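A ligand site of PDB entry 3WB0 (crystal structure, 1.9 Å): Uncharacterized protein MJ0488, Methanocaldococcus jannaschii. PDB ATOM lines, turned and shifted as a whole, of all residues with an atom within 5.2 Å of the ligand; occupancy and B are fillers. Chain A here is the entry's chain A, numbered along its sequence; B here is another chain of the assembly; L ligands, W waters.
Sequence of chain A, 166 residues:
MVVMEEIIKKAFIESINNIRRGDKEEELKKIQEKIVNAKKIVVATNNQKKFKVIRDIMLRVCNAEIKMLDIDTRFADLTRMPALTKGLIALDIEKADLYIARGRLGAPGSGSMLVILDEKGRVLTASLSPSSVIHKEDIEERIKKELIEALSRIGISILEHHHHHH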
ATOM      1  N   LYS A  50      -4.048  -8.039  12.103  1.00  0.00           N
ATOM      2  CA  LYS A  50      -3.993  -9.025  13.207  1.00  0.00           C
ATOM      3  C   LYS A  50      -2.570  -9.605  13.348  1.00  0.00           C
ATOM      4  O   LYS A  50      -2.003  -9.674  14.452  1.00  0.00           O
ATOM      5  CB  LYS A  50      -5.026 -10.150  13.038  1.00  0.00           C
ATOM      6  CG  LYS A  50      -6.493  -9.710  13.078  1.00  0.00           C
ATOM      7  CD  LYS A  50      -7.499 -10.793  12.678  1.00  0.00           C
ATOM      8  CE  LYS A  50      -8.126 -11.456  13.890  1.00  0.00           C
ATOM      9  NZ  LYS A  50      -9.080 -12.550  13.524  1.00  0.00           N
ATOM     10  N   ASP A  77     -15.167 -20.138  11.148  1.00  0.00           N
ATOM     11  CA  ASP A  77     -16.306 -19.526  11.827  1.00  0.00           C
ATOM     12  C   ASP A  77     -17.674 -20.246  11.674  1.00  0.00           C
ATOM     13  O   ASP A  77     -18.660 -19.794  12.237  1.00  0.00           O
ATOM     14  CB  ASP A  77     -16.403 -18.041  11.572  1.00  0.00           C
ATOM     15  CG  ASP A  77     -15.050 -17.325  11.694  1.00  0.00           C
ATOM     16  OD1 ASP A  77     -14.133 -17.849  12.434  1.00  0.00           O
ATOM     17  OD2 ASP A  77     -14.931 -16.266  11.000  1.00  0.00           O
ATOM     18  N   LYS A  86      -9.120 -22.475  13.962  1.00  0.00           N
ATOM     19  CA  LYS A  86      -8.183 -21.733  13.159  1.00  0.00           C
ATOM     20  C   LYS A  86      -6.804 -22.199  13.544  1.00  0.00           C
ATOM     21  O   LYS A  86      -5.960 -22.353  12.649  1.00  0.00           O
ATOM     22  CB  LYS A  86      -8.224 -20.208  13.438  1.00  0.00           C
ATOM     23  CG  LYS A  86      -9.495 -19.485  12.963  1.00  0.00           C
ATOM     24  CD  LYS A  86      -9.252 -18.018  13.373  1.00  0.00           C
ATOM     25  CE  LYS A  86     -10.457 -17.103  13.040  1.00  0.00           C
ATOM     26  NZ  LYS A  86     -10.670 -17.028  11.563  1.00  0.00           N
ATOM     27  N   ARG A 102      -6.637 -16.283  16.663  1.00  0.00           N
ATOM     28  CA  ARG A 102      -7.550 -15.314  17.369  1.00  0.00           C
ATOM     29  C   ARG A 102      -8.864 -15.211  16.570  1.00  0.00           C
ATOM     30  O   ARG A 102      -8.833 -14.958  15.358  1.00  0.00           O
ATOM     31  CB  ARG A 102      -6.849 -13.915  17.577  1.00  0.00           C
ATOM     32  CG  ARG A 102      -7.631 -12.953  18.537  1.00  0.00           C
ATOM     33  CD  ARG A 102      -8.877 -12.313  17.926  1.00  0.00           C
ATOM     34  NE  ARG A 102      -9.417 -11.315  18.901  1.00  0.00           N
ATOM     35  CZ  ARG A 102     -10.372 -10.408  18.658  1.00  0.00           C
ATOM     36  NH1 ARG A 102     -10.770  -9.572  19.658  1.00  0.00           N
ATOM     37  NH2 ARG A 102     -10.932 -10.313  17.451  1.00  0.00           N
ATOM     38  N   GLY A 103      -9.979 -15.460  17.227  1.00  0.00           N
ATOM     39  CA  GLY A 103     -11.337 -15.437  16.606  1.00  0.00           C
ATOM     40  C   GLY A 103     -12.408 -15.523  17.671  1.00  0.00           C
ATOM     41  O   GLY A 103     -12.192 -15.226  18.836  1.00  0.00           O
ATOM     42  N   ARG A 104     -13.582 -15.949  17.259  1.00  0.00           N
ATOM     43  CA  ARG A 104     -14.743 -16.145  18.124  1.00  0.00           C
ATOM     44  C   ARG A 104     -14.540 -17.403  18.988  1.00  0.00           C
ATOM     45  O   ARG A 104     -13.928 -18.394  18.543  1.00  0.00           O
ATOM     46  CB  ARG A 104     -16.062 -16.211  17.297  1.00  0.00           C
ATOM     47  CG  ARG A 104     -17.332 -16.346  18.090  1.00  0.00           C
ATOM     48  CD  ARG A 104     -18.545 -16.138  17.203  1.00  0.00           C
ATOM     49  NE  ARG A 104     -18.916 -17.396  16.513  1.00  0.00           N
ATOM     50  CZ  ARG A 104     -19.075 -17.512  15.194  1.00  0.00           C
ATOM     51  NH1 ARG A 104     -19.021 -16.420  14.391  1.00  0.00           N
ATOM     52  NH2 ARG A 104     -19.366 -18.697  14.668  1.00  0.00           N
ATOM     53  N   SER A 110     -20.608 -14.843  21.441  1.00  0.00           N
ATOM     54  CA  SER A 110     -19.825 -15.266  22.592  1.00  0.00           C
ATOM     55  C   SER A 110     -18.463 -14.526  22.790  1.00  0.00           C
ATOM     56  O   SER A 110     -17.680 -14.918  23.634  1.00  0.00           O
ATOM     57  CB  SER A 110     -19.607 -16.769  22.515  1.00  0.00           C
ATOM     58  OG  SER A 110     -18.836 -17.117  21.365  1.00  0.00           O
ATOM     59  N   GLY A 111     -18.157 -13.492  22.023  1.00  0.00           N
ATOM     60  CA  GLY A 111     -16.897 -12.789  22.274  1.00  0.00           C
ATOM     61  C   GLY A 111     -15.738 -13.548  21.662  1.00  0.00           C
ATOM     62  O   GLY A 111     -15.955 -14.477  20.875  1.00  0.00           O
ATOM     63  N   SER A 112     -14.512 -13.206  22.054  1.00  0.00           N
ATOM     64  CA  SER A 112     -13.380 -13.632  21.277  1.00  0.00           C
ATOM     65  C   SER A 112     -12.445 -14.436  22.173  1.00  0.00           C
ATOM     66  O   SER A 112     -12.522 -14.316  23.428  1.00  0.00           O
ATOM     67  CB  SER A 112     -12.568 -12.392  20.841  1.00  0.00           C
ATOM     68  OG  SER A 112     -11.998 -11.837  22.031  1.00  0.00           O
ATOM     69  N   PRO A 130     -14.690  -9.532  25.999  1.00  0.00           N
ATOM     70  CA  PRO A 130     -16.122  -9.553  25.869  1.00  0.00           C
ATOM     71  C   PRO A 130     -16.515  -9.338  24.426  1.00  0.00           C
ATOM     72  O   PRO A 130     -15.701  -8.893  23.604  1.00  0.00           O
ATOM     73  CB  PRO A 130     -16.550  -8.347  26.701  1.00  0.00           C
ATOM     74  CG  PRO A 130     -15.467  -8.187  27.686  1.00  0.00           C
ATOM     75  CD  PRO A 130     -14.240  -8.467  26.928  1.00  0.00           C
ATOM     76  N   SER A 131     -17.773  -9.615  24.145  1.00  0.00           N
ATOM     77  CA  SER A 131     -18.262  -9.452  22.857  1.00  0.00           C
ATOM     78  C   SER A 131     -18.071  -7.985  22.410  1.00  0.00           C
ATOM     79  O   SER A 131     -18.319  -7.080  23.163  1.00  0.00           O
ATOM     80  CB  SER A 131     -19.742  -9.782  22.880  1.00  0.00           C
ATOM     81  OG  SER A 131     -20.210  -9.635  21.577  1.00  0.00           O
ATOM     82  N   SER A 132     -17.678  -7.781  21.168  1.00  0.00           N
ATOM     83  CA  SER A 132     -17.477  -6.460  20.652  1.00  0.00           C
ATOM     84  C   SER A 132     -18.716  -5.580  20.636  1.00  0.00           C
ATOM     85  O   SER A 132     -18.559  -4.357  20.661  1.00  0.00           O
ATOM     86  CB  SER A 132     -16.880  -6.512  19.256  1.00  0.00           C
ATOM     87  OG  SER A 132     -17.676  -7.299  18.340  1.00  0.00           O
ATOM     88  N   VAL A 133     -19.913  -6.180  20.657  1.00  0.00           N
ATOM     89  CA  VAL A 133     -21.192  -5.495  20.756  1.00  0.00           C
ATOM     90  C   VAL A 133     -21.194  -4.653  22.044  1.00  0.00           C
ATOM     91  O   VAL A 133     -21.877  -3.628  22.126  1.00  0.00           O
ATOM     92  CB  VAL A 133     -22.370  -6.501  20.871  1.00  0.00           C
ATOM     93  CG1 VAL A 133     -23.643  -5.836  21.357  1.00  0.00           C
ATOM     94  CG2 VAL A 133     -22.566  -7.254  19.569  1.00  0.00           C
ATOM     95  N   HIS A 135     -17.886  -3.991  24.450  1.00  0.00           N
ATOM     96  CA  HIS A 135     -16.669  -3.182  24.605  1.00  0.00           C
ATOM     97  C   HIS A 135     -16.400  -2.085  23.539  1.00  0.00           C
ATOM     98  O   HIS A 135     -15.804  -1.056  23.870  1.00  0.00           O
ATOM     99  CB  HIS A 135     -15.431  -4.068  24.809  1.00  0.00           C
ATOM    100  CG  HIS A 135     -14.982  -4.826  23.594  1.00  0.00           C
ATOM    101  ND1 HIS A 135     -14.281  -4.235  22.556  1.00  0.00           N
ATOM    102  CD2 HIS A 135     -15.078  -6.137  23.262  1.00  0.00           C
ATOM    103  CE1 HIS A 135     -13.977  -5.148  21.636  1.00  0.00           C
ATOM    104  NE2 HIS A 135     -14.438  -6.313  22.049  1.00  0.00           N
ATOM    105  N   LYS A 136     -16.851  -2.295  22.287  1.00  0.00           N
ATOM    106  CA  LYS A 136     -16.557  -1.424  21.110  1.00  0.00           C
ATOM    107  C   LYS A 136     -15.109  -0.809  20.904  1.00  0.00           C
ATOM    108  O   LYS A 136     -14.964   0.313  20.375  1.00  0.00           O
ATOM    109  CB  LYS A 136     -17.614  -0.327  20.967  1.00  0.00           C
ATOM    110  CG  LYS A 136     -17.602   0.352  19.588  1.00  0.00           C
ATOM    111  CD  LYS A 136     -18.817   0.046  18.704  1.00  0.00           C
ATOM    112  CE  LYS A 136     -20.099   0.697  19.214  1.00  0.00           C
ATOM    113  NZ  LYS A 136     -21.034  -0.196  19.978  1.00  0.00           N
ATOM    114  N   GLU A 137     -14.055  -1.547  21.265  1.00  0.00           N
ATOM    115  CA  GLU A 137     -12.648  -1.055  21.095  1.00  0.00           C
ATOM    116  C   GLU A 137     -12.051  -1.516  19.740  1.00  0.00           C
ATOM    117  O   GLU A 137     -12.522  -2.508  19.158  1.00  0.00           O
ATOM    118  CB  GLU A 137     -11.754  -1.585  22.219  1.00  0.00           C
ATOM    119  CG  GLU A 137     -11.944  -1.018  23.613  1.00  0.00           C
ATOM    120  CD  GLU A 137     -11.121  -1.815  24.644  1.00  0.00           C
ATOM    121  OE1 GLU A 137      -9.859  -1.881  24.524  1.00  0.00           O
ATOM    122  OE2 GLU A 137     -11.732  -2.414  25.551  1.00  0.00           O
ATOM    123  N   ASP A 138     -11.038  -0.778  19.248  1.00  0.00           N
ATOM    124  CA  ASP A 138     -10.294  -1.137  18.023  1.00  0.00           C
ATOM    125  C   ASP A 138      -9.842  -2.580  18.117  1.00  0.00           C
ATOM    126  O   ASP A 138      -9.304  -3.003  19.152  1.00  0.00           O
ATOM    127  CB  ASP A 138      -9.059  -0.239  17.792  1.00  0.00           C
ATOM    128  CG  ASP A 138      -8.532  -0.289  16.339  1.00  0.00           C
ATOM    129  OD1 ASP A 138      -8.040  -1.358  15.858  1.00  0.00           O
ATOM    130  OD2 ASP A 138      -8.603   0.764  15.652  1.00  0.00           O
ATOM    131  N   ILE A 139     -10.022  -3.331  17.026  1.00  0.00           N
ATOM    132  CA  ILE A 139      -9.550  -4.719  17.026  1.00  0.00           C
ATOM    133  C   ILE A 139      -8.076  -4.850  17.406  1.00  0.00           C
ATOM    134  O   ILE A 139      -7.690  -5.794  18.079  1.00  0.00           O
ATOM    135  CB  ILE A 139      -9.883  -5.485  15.720  1.00  0.00           C
ATOM    136  CG1 ILE A 139      -9.858  -7.009  15.989  1.00  0.00           C
ATOM    137  CG2 ILE A 139      -8.937  -5.124  14.557  1.00  0.00           C
ATOM    138  CD1 ILE A 139     -10.510  -7.778  14.853  1.00  0.00           C
ATOM    139  N   ARG A 142      -7.679  -4.553  21.161  1.00  0.00           N
ATOM    140  CA  ARG A 142      -8.201  -5.794  21.787  1.00  0.00           C
ATOM    141  C   ARG A 142      -7.160  -6.973  21.697  1.00  0.00           C
ATOM    142  O   ARG A 142      -6.798  -7.591  22.705  1.00  0.00           O
ATOM    143  CB  ARG A 142      -9.524  -6.125  21.093  1.00  0.00           C
ATOM    144  CG  ARG A 142     -10.699  -6.475  21.984  1.00  0.00           C
ATOM    145  CD  ARG A 142     -10.876  -5.577  23.213  1.00  0.00           C
ATOM    146  NE  ARG A 142     -10.496  -6.392  24.353  1.00  0.00           N
ATOM    147  CZ  ARG A 142     -10.813  -6.152  25.624  1.00  0.00           C
ATOM    148  NH1 ARG A 142     -11.528  -5.091  25.980  1.00  0.00           N
ATOM    149  NH2 ARG A 142     -10.413  -7.011  26.542  1.00  0.00           N
ATOM    150  N   GLU A 146      -5.293  -8.979  24.590  1.00  0.00           N
ATOM    151  CA  GLU A 146      -5.498 -10.415  24.654  1.00  0.00           C
ATOM    152  C   GLU A 146      -4.179 -11.165  24.698  1.00  0.00           C
ATOM    153  O   GLU A 146      -4.014 -12.050  25.525  1.00  0.00           O
ATOM    154  CB  GLU A 146      -6.353 -10.995  23.513  1.00  0.00           C
ATOM    155  CG  GLU A 146      -7.836 -10.690  23.603  1.00  0.00           C
ATOM    156  CD  GLU A 146      -8.550 -10.756  22.252  1.00  0.00           C
ATOM    157  OE1 GLU A 146      -7.977 -11.241  21.272  1.00  0.00           O
ATOM    158  OE2 GLU A 146      -9.697 -10.280  22.142  1.00  0.00           O
ATOM    159  N   SER B  15     -20.654 -15.260   7.200  1.00  0.00           N
ATOM    160  CA  SER B  15     -19.296 -15.799   7.103  1.00  0.00           C
ATOM    161  C   SER B  15     -18.955 -16.372   5.684  1.00  0.00           C
ATOM    162  O   SER B  15     -17.927 -16.030   5.076  1.00  0.00           O
ATOM    163  CB  SER B  15     -19.023 -16.835   8.213  1.00  0.00           C
ATOM    164  OG  SER B  15     -18.989 -16.208   9.486  1.00  0.00           O
ATOM    165  N   ARG B  20     -19.181 -10.968   7.409  1.00  0.00           N
ATOM    166  CA  ARG B  20     -19.309 -11.074   8.853  1.00  0.00           C
ATOM    167  C   ARG B  20     -18.433 -10.001   9.554  1.00  0.00           C
ATOM    168  O   ARG B  20     -17.209 -10.056   9.476  1.00  0.00           O
ATOM    169  CB  ARG B  20     -18.883 -12.483   9.283  1.00  0.00           C
ATOM    170  CG  ARG B  20     -18.884 -12.759  10.766  1.00  0.00           C
ATOM    171  CD  ARG B  20     -20.296 -12.801  11.338  1.00  0.00           C
ATOM    172  NE  ARG B  20     -20.302 -13.057  12.808  1.00  0.00           N
ATOM    173  CZ  ARG B  20     -21.425 -13.000  13.519  1.00  0.00           C
ATOM    174  NH1 ARG B  20     -22.572 -12.685  12.896  1.00  0.00           N
ATOM    175  NH2 ARG B  20     -21.387 -13.235  14.811  1.00  0.00           N
ATOM    176  N   ARG B  21     -19.049  -9.079  10.293  1.00  0.00           N
ATOM    177  CA  ARG B  21     -18.287  -8.043  11.007  1.00  0.00           C
ATOM    178  C   ARG B  21     -18.454  -8.149  12.534  1.00  0.00           C
ATOM    179  O   ARG B  21     -18.746  -7.168  13.221  1.00  0.00           O
ATOM    180  CB  ARG B  21     -18.659  -6.651  10.502  1.00  0.00           C
ATOM    181  CG  ARG B  21     -18.455  -6.496   8.990  1.00  0.00           C
ATOM    182  CD  ARG B  21     -17.101  -5.873   8.602  1.00  0.00           C
ATOM    183  NE  ARG B  21     -15.914  -6.666   8.927  1.00  0.00           N
ATOM    184  CZ  ARG B  21     -15.476  -7.745   8.254  1.00  0.00           C
ATOM    185  NH1 ARG B  21     -14.380  -8.379   8.653  1.00  0.00           N
ATOM    186  NH2 ARG B  21     -16.145  -8.240   7.188  1.00  0.00           N
ATOM    187  N   GLY B  22     -18.240  -9.362  13.007  1.00  0.00           N
ATOM    188  CA  GLY B  22     -18.259  -9.736  14.441  1.00  0.00           C
ATOM    189  C   GLY B  22     -19.664  -9.992  14.940  1.00  0.00           C
ATOM    190  O   GLY B  22     -20.639 -10.090  14.134  1.00  0.00           O
ATOM    191  N   ASP B  23     -19.771 -10.082  16.256  1.00  0.00           N
ATOM    192  CA  ASP B  23     -21.037 -10.377  16.946  1.00  0.00           C
ATOM    193  C   ASP B  23     -22.038  -9.279  16.738  1.00  0.00           C
ATOM    194  O   ASP B  23     -21.678  -8.125  16.585  1.00  0.00           O
ATOM    195  CB  ASP B  23     -20.821 -10.493  18.473  1.00  0.00           C
ATOM    196  CG  ASP B  23     -19.981 -11.713  18.882  1.00  0.00           C
ATOM    197  OD1 ASP B  23     -19.864 -12.668  18.068  1.00  0.00           O
ATOM    198  OD2 ASP B  23     -19.481 -11.727  20.055  1.00  0.00           O
HETATM  199  N1  LIG L   1     -17.543 -12.827  16.597  1.00  0.00           N
HETATM  200  C1  LIG L   1     -17.445 -13.354  15.281  1.00  0.00           C
HETATM  201  O1  LIG L   1     -18.541 -13.662  14.567  1.00  0.00           O
HETATM  202  C2  LIG L   1     -16.152 -13.554  14.579  1.00  0.00           C
HETATM  203  C3  LIG L   1     -16.113 -14.122  13.161  1.00  0.00           C
HETATM  204  C4  LIG L   1     -14.932 -13.155  15.326  1.00  0.00           C
HETATM  205  C5  LIG L   1     -15.102 -12.649  16.762  1.00  0.00           C
HETATM  206  C6  LIG L   1     -13.850 -12.296  17.565  1.00  0.00           C
HETATM  207  C7  LIG L   1     -16.435 -12.495  17.329  1.00  0.00           C
HETATM  208  C8  LIG L   1     -16.621 -11.938  18.741  1.00  0.00           C
HETATM  209  C9  LIG L   1     -16.870 -10.460  18.745  1.00  0.00           C
HETATM  210  O2  LIG L   1     -16.547  -9.838  19.785  1.00  0.00           O
HETATM  211  O3  LIG L   1     -17.397  -9.874  17.748  1.00  0.00           O
HETATM  212  O4  LIG L   1     -13.696 -13.401  14.746  1.00  0.00           O
HETATM  213  P1  LIG L   1     -12.597 -12.389  14.140  1.00  0.00           P
HETATM  214  O5  LIG L   1     -11.426 -12.039  15.071  1.00  0.00           O
HETATM  215  O6  LIG L   1     -12.170 -13.078  12.850  1.00  0.00           O
HETATM  216  O7  LIG L   1     -13.485 -11.110  13.714  1.00  0.00           O
HETATM  217  C10 LIG L   1     -14.302 -11.003  12.550  1.00  0.00           C
HETATM  218  C11 LIG L   1     -14.595  -9.482  12.409  1.00  0.00           C
HETATM  219  C12 LIG L   1     -13.446  -8.510  12.492  1.00  0.00           C
HETATM  220  O8  LIG L   1     -13.036  -8.273  11.155  1.00  0.00           O
HETATM  221  C13 LIG L   1     -14.107  -7.228  12.981  1.00  0.00           C
HETATM  222  O9  LIG L   1     -14.857  -6.721  11.842  1.00  0.00           O
HETATM  223  C14 LIG L   1     -15.105  -7.742  14.014  1.00  0.00           C
HETATM  224  O10 LIG L   1     -15.431  -9.050  13.502  1.00  0.00           O
HETATM  225  N2  LIG L   1     -14.413  -7.842  15.334  1.00  0.00           N
HETATM  226  C15 LIG L   1     -13.972  -8.975  15.927  1.00  0.00           C
HETATM  227  N3  LIG L   1     -13.344  -8.683  17.103  1.00  0.00           N
HETATM  228  C16 LIG L   1     -13.375  -7.351  17.274  1.00  0.00           C
HETATM  229  C17 LIG L   1     -14.073  -6.784  16.090  1.00  0.00           C
HETATM  230  C18 LIG L   1     -12.907  -6.389  18.317  1.00  0.00           C
HETATM  231  O11 LIG L   1     -12.252  -6.762  19.335  1.00  0.00           O
HETATM  232  N4  LIG L   1     -13.124  -5.099  18.067  1.00  0.00           N
HETATM  233  C19 LIG L   1     -13.788  -4.629  16.983  1.00  0.00           C
HETATM  234  N5  LIG L   1     -14.245  -5.427  15.978  1.00  0.00           N
HETATM  235  N6  LIG L   1     -13.993  -3.283  16.913  1.00  0.00           N
HETATM  236  O   HOH W   1     -13.513 -16.408  14.283  1.00  0.00           O
HETATM  237  O   HOH W   2     -12.507 -14.982  11.030  1.00  0.00           O
HETATM  238  O   HOH W   3     -14.351  -9.210  21.449  1.00  0.00           O
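Water W2 lies within hydrogen-bond range of O6 of the ligand (2.7 Å), OD2 of Asp 77 (2.7 Å) and NZ of Lys 86 (2.8 Å). Water W3 lies within hydrogen-bond range of the backbone carbonyl oxygen of Pro 130 (2.6 Å), an oxygen (O2) of the ligand (2.8 Å) and a ring nitrogen (NE2) of His 135 (3.0 Å). Water W1 lies within hydrogen-bond range of OD1 of Asp 77 (2.4 Å), N of Arg 104 (3.0 Å) and O4 of the ligand (3.0 Å).
Asp 77 touches the ligand. Gly 103 touches the ligand (C to C6, 3.5 Å). Gly 111 touches the ligand (O to C8, 3.4 Å). Ser 112 touches the ligand (CB to C6, 3.5 Å). CA of Ser 131 touches O2 of the ligand, 3.5 Å away. CE1 of His 135 touches O11 of the ligand, 3.3 Å away. N of Ile 139 touches N4 of the ligand, at 3.7 Å. Arg 142 touches the ligand (CG to O11, 3.1 Å). Hydrophobic or aromatic side chains that line the ligand: His 135 and Ile 139. Of the 25 residues printed, 17 come within 4 Å of the ligand. The nearest printed residue that does not touch the ligand is Pro 130 (4.02 Å).
The side-chain carboxylate of Asp 23 of chain B lies within hydrogen-bond range of a nitrogen (N1) of the ligand (2.8 Å). O of Glu 137 is in hydrogen-bond range of N6 of the ligand. O2 of the ligand is in hydrogen-bond range of N of Ser 132 (2.7 Å). The side-chain amino group (NZ) of Lys 50 is in salt-bridge range of an oxygen (O5) of the ligand. The guanidinium group (NH2) of Arg 102 lies within salt-bridge range of an oxygen (O5) of the ligand, at 3.0 Å. An oxygen (O1) of the ligand sits at hydrogen-bond distance from the guanidinium group (NE) of Arg 20 of chain B, 2.6 Å away. NH1 of Arg 104 lies within hydrogen-bond range of O1 of the ligand (2.8 Å). The backbone NH (N) of Asp 23 of chain B lies within hydrogen-bond range of an oxygen (O3) of the ligand (2.8 Å). The side-chain hydroxyl of Ser 132 is in hydrogen-bond range of an oxygen (O3) of the ligand (2.7 Å). An oxygen (O8) of the ligand is in hydrogen-bond range of the guanidinium group (NH1) of Arg 21 of chain B (2.8 Å). The backbone NH (N) of Gly 22 of chain B sits at hydrogen-bond distance from an oxygen (O10) of the ligand, 2.9 Å away.
O of Arg 102 lies within hydrogen-bond range of NZ of Lys 50. The side-chain hydroxyl (OG) of Ser 131 lies within hydrogen-bond range of the side-chain carboxylate (OD2) of Asp 23 of chain B, 2.7 Å away. The guanidinium group (NH2) of Arg 104 lies within hydrogen-bond range of the backbone carbonyl oxygen (O) of Asp 77, at 2.8 Å. The guanidinium group (NE) of Arg 102 is in salt-bridge range of the side-chain carboxylate (OE1) of Glu 146 (2.8 Å). OD1 of Asp 77 is in salt-bridge range of NZ of Lys 86, 3.7 Å away. O of Gly 22 of chain B lies close to NE of Arg 20 of chain B, 3.3 Å away. The side-chain carboxylate (OE2) of Glu 137 lies within salt-bridge range of the guanidinium group (NH1) of Arg 142 (2.7 Å). OD2 of Asp 23 of chain B lies within hydrogen-bond range of N of Gly 111 (3.0 Å).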
